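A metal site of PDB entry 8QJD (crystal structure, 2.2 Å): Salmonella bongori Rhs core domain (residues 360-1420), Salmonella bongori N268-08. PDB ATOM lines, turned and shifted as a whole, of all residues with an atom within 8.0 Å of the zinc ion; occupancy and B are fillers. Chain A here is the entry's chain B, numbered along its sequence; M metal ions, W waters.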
ATOM      1  N   THR A  58     -31.518 -22.392 -20.735  1.00  0.00           N
ATOM      2  CA  THR A  58     -31.879 -22.800 -19.381  1.00  0.00           C
ATOM      3  C   THR A  58     -30.705 -23.469 -18.701  1.00  0.00           C
ATOM      4  O   THR A  58     -30.069 -24.361 -19.296  1.00  0.00           O
ATOM      5  CB  THR A  58     -33.091 -23.738 -19.381  1.00  0.00           C
ATOM      6  OG1 THR A  58     -34.204 -23.086 -20.014  1.00  0.00           O
ATOM      7  CG2 THR A  58     -33.492 -24.096 -17.954  1.00  0.00           C
ATOM      8  N   VAL A  59     -30.406 -23.067 -17.470  1.00  0.00           N
ATOM      9  CA  VAL A  59     -29.413 -23.742 -16.643  1.00  0.00           C
ATOM     10  C   VAL A  59     -30.013 -25.027 -16.099  1.00  0.00           C
ATOM     11  O   VAL A  59     -31.172 -25.065 -15.686  1.00  0.00           O
ATOM     12  CB  VAL A  59     -28.918 -22.825 -15.513  1.00  0.00           C
ATOM     13  CG1 VAL A  59     -27.873 -23.540 -14.674  1.00  0.00           C
ATOM     14  CG2 VAL A  59     -28.341 -21.545 -16.091  1.00  0.00           C
ATOM     15  N   HIS A  60     -29.221 -26.111 -16.119  1.00  0.00           N
ATOM     16  CA  HIS A  60     -29.608 -27.431 -15.618  1.00  0.00           C
ATOM     17  C   HIS A  60     -28.370 -28.066 -14.969  1.00  0.00           C
ATOM     18  O   HIS A  60     -27.755 -28.990 -15.477  1.00  0.00           O
ATOM     19  CB  HIS A  60     -30.176 -28.310 -16.736  1.00  0.00           C
ATOM     20  CG  HIS A  60     -30.522 -29.702 -16.303  1.00  0.00           C
ATOM     21  ND1 HIS A  60     -30.762 -30.723 -17.201  1.00  0.00           N
ATOM     22  CD2 HIS A  60     -30.638 -30.254 -15.068  1.00  0.00           C
ATOM     23  CE1 HIS A  60     -31.035 -31.838 -16.543  1.00  0.00           C
ATOM     24  NE2 HIS A  60     -30.969 -31.575 -15.246  1.00  0.00           N
ATOM     25  N   GLY A  61     -27.982 -27.522 -13.811  1.00  0.00           N
ATOM     26  CA  GLY A  61     -26.805 -28.018 -13.140  1.00  0.00           C
ATOM     27  C   GLY A  61     -25.540 -27.444 -13.739  1.00  0.00           C
ATOM     28  O   GLY A  61     -25.250 -26.261 -13.590  1.00  0.00           O
ATOM     29  N   ASN A  62     -24.773 -28.292 -14.423  1.00  0.00           N
ATOM     30  CA  ASN A  62     -23.524 -27.899 -15.064  1.00  0.00           C
ATOM     31  C   ASN A  62     -23.654 -27.736 -16.568  1.00  0.00           C
ATOM     32  O   ASN A  62     -22.662 -27.411 -17.226  1.00  0.00           O
ATOM     33  CB  ASN A  62     -22.410 -28.897 -14.752  1.00  0.00           C
ATOM     34  CG  ASN A  62     -22.123 -29.016 -13.266  1.00  0.00           C
ATOM     35  OD1 ASN A  62     -21.483 -28.145 -12.681  1.00  0.00           O
ATOM     36  ND2 ASN A  62     -22.593 -30.106 -12.659  1.00  0.00           N
ATOM     37  N   ASP A  63     -24.829 -27.980 -17.140  1.00  0.00           N
ATOM     38  CA  ASP A  63     -25.032 -27.810 -18.569  1.00  0.00           C
ATOM     39  C   ASP A  63     -26.091 -26.748 -18.843  1.00  0.00           C
ATOM     40  O   ASP A  63     -26.919 -26.433 -17.996  1.00  0.00           O
ATOM     41  CB  ASP A  63     -25.411 -29.131 -19.252  1.00  0.00           C
ATOM     42  CG  ASP A  63     -26.642 -29.777 -18.634  1.00  0.00           C
ATOM     43  OD1 ASP A  63     -27.737 -29.179 -18.710  1.00  0.00           O
ATOM     44  OD2 ASP A  63     -26.523 -30.886 -18.094  1.00  0.00           O
ATOM     45  N   MET A  64     -26.027 -26.205 -20.058  1.00  0.00           N
ATOM     46  CA  MET A  64     -26.953 -25.189 -20.528  1.00  0.00           C
ATOM     47  C   MET A  64     -27.811 -25.772 -21.648  1.00  0.00           C
ATOM     48  O   MET A  64     -27.278 -26.357 -22.595  1.00  0.00           O
ATOM     49  CB  MET A  64     -26.203 -23.955 -21.019  1.00  0.00           C
ATOM     50  CG  MET A  64     -27.072 -22.776 -21.377  1.00  0.00           C
ATOM     51  SD  MET A  64     -27.688 -21.900 -19.922  1.00  0.00           S
ATOM     52  CE  MET A  64     -26.157 -21.377 -19.152  1.00  0.00           C
ATOM     53  N   HIS A  65     -29.130 -25.625 -21.536  1.00  0.00           N
ATOM     54  CA  HIS A  65     -30.057 -26.160 -22.529  1.00  0.00           C
ATOM     55  C   HIS A  65     -30.468 -25.041 -23.472  1.00  0.00           C
ATOM     56  O   HIS A  65     -30.983 -24.007 -23.036  1.00  0.00           O
ATOM     57  CB  HIS A  65     -31.299 -26.749 -21.858  1.00  0.00           C
ATOM     58  CG  HIS A  65     -31.037 -28.002 -21.091  1.00  0.00           C
ATOM     59  ND1 HIS A  65     -32.047 -28.886 -20.757  1.00  0.00           N
ATOM     60  CD2 HIS A  65     -29.907 -28.515 -20.578  1.00  0.00           C
ATOM     61  CE1 HIS A  65     -31.530 -29.897 -20.077  1.00  0.00           C
ATOM     62  NE2 HIS A  65     -30.230 -29.701 -19.956  1.00  0.00           N
ATOM     63  N   ASP A  73     -33.560 -29.505 -27.990  1.00  0.00           N
ATOM     64  CA  ASP A  73     -32.702 -29.063 -26.900  1.00  0.00           C
ATOM     65  C   ASP A  73     -31.257 -29.414 -27.216  1.00  0.00           C
ATOM     66  O   ASP A  73     -30.939 -30.584 -27.441  1.00  0.00           O
ATOM     67  CB  ASP A  73     -33.127 -29.684 -25.572  1.00  0.00           C
ATOM     68  CG  ASP A  73     -34.233 -28.907 -24.889  1.00  0.00           C
ATOM     69  OD1 ASP A  73     -34.662 -27.868 -25.438  1.00  0.00           O
ATOM     70  OD2 ASP A  73     -34.675 -29.325 -23.792  1.00  0.00           O
ATOM     71  N   LEU A  74     -30.398 -28.414 -27.239  1.00  0.00           N
ATOM     72  CA  LEU A  74     -28.964 -28.598 -27.409  1.00  0.00           C
ATOM     73  C   LEU A  74     -28.286 -28.308 -26.086  1.00  0.00           C
ATOM     74  O   LEU A  74     -28.600 -27.328 -25.411  1.00  0.00           O
ATOM     75  CB  LEU A  74     -28.418 -27.680 -28.504  1.00  0.00           C
ATOM     76  CG  LEU A  74     -28.972 -27.902 -29.913  1.00  0.00           C
ATOM     77  CD1 LEU A  74     -28.485 -26.822 -30.864  1.00  0.00           C
ATOM     78  CD2 LEU A  74     -28.598 -29.282 -30.424  1.00  0.00           C
ATOM     79  N   TYR A  75     -27.349 -29.174 -25.708  1.00  0.00           N
ATOM     80  CA  TYR A  75     -26.710 -29.096 -24.410  1.00  0.00           C
ATOM     81  C   TYR A  75     -25.289 -28.571 -24.553  1.00  0.00           C
ATOM     82  O   TYR A  75     -24.558 -28.964 -25.470  1.00  0.00           O
ATOM     83  CB  TYR A  75     -26.722 -30.462 -23.729  1.00  0.00           C
ATOM     84  CG  TYR A  75     -28.082 -31.117 -23.769  1.00  0.00           C
ATOM     85  CD1 TYR A  75     -29.066 -30.797 -22.832  1.00  0.00           C
ATOM     86  CD2 TYR A  75     -28.409 -32.047 -24.764  1.00  0.00           C
ATOM     87  CE1 TYR A  75     -30.316 -31.389 -22.873  1.00  0.00           C
ATOM     88  CE2 TYR A  75     -29.659 -32.639 -24.805  1.00  0.00           C
ATOM     89  CZ  TYR A  75     -30.603 -32.305 -23.861  1.00  0.00           C
ATOM     90  OH  TYR A  75     -31.849 -32.899 -23.911  1.00  0.00           O
ATOM     91  N   TYR A  76     -24.908 -27.668 -23.651  1.00  0.00           N
ATOM     92  CA  TYR A  76     -23.561 -27.116 -23.575  1.00  0.00           C
ATOM     93  C   TYR A  76     -23.108 -27.188 -22.138  1.00  0.00           C
ATOM     94  O   TYR A  76     -23.801 -26.696 -21.244  1.00  0.00           O
ATOM     95  CB  TYR A  76     -23.527 -25.657 -24.045  1.00  0.00           C
ATOM     96  CG  TYR A  76     -24.059 -25.433 -25.438  1.00  0.00           C
ATOM     97  CD1 TYR A  76     -25.428 -25.325 -25.676  1.00  0.00           C
ATOM     98  CD2 TYR A  76     -23.200 -25.309 -26.526  1.00  0.00           C
ATOM     99  CE1 TYR A  76     -25.914 -25.116 -26.951  1.00  0.00           C
ATOM    100  CE2 TYR A  76     -23.681 -25.102 -27.809  1.00  0.00           C
ATOM    101  CZ  TYR A  76     -25.043 -25.007 -28.006  1.00  0.00           C
ATOM    102  OH  TYR A  76     -25.529 -24.798 -29.281  1.00  0.00           O
HETATM  103 ZN    ZN M   1     -29.064 -30.992 -18.795  1.00  0.00          ZN
HETATM  104  O   HOH W   1     -29.073 -33.066 -20.523  1.00  0.00           O
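The zinc ion is bound by a ring nitrogen (NE2) of His 65, the side-chain carboxylate of Asp 63 and a ring nitrogen (ND1) of His 60.
The zinc ion has three donor atoms within binding distance.
Slightly farther from the zinc ion lies OD2 of Asp 63 (2.6 Å).
Slightly farther from the zinc ion lies water W1 (2.7 Å).
The backbone NH (N) of His 65 lies within hydrogen-bond range of the backbone carbonyl oxygen (O) of Thr 58, at 2.7 Å.
Three residues have an atom within 4 Å of the zinc ion: His 60, Asp 63 and His 65.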
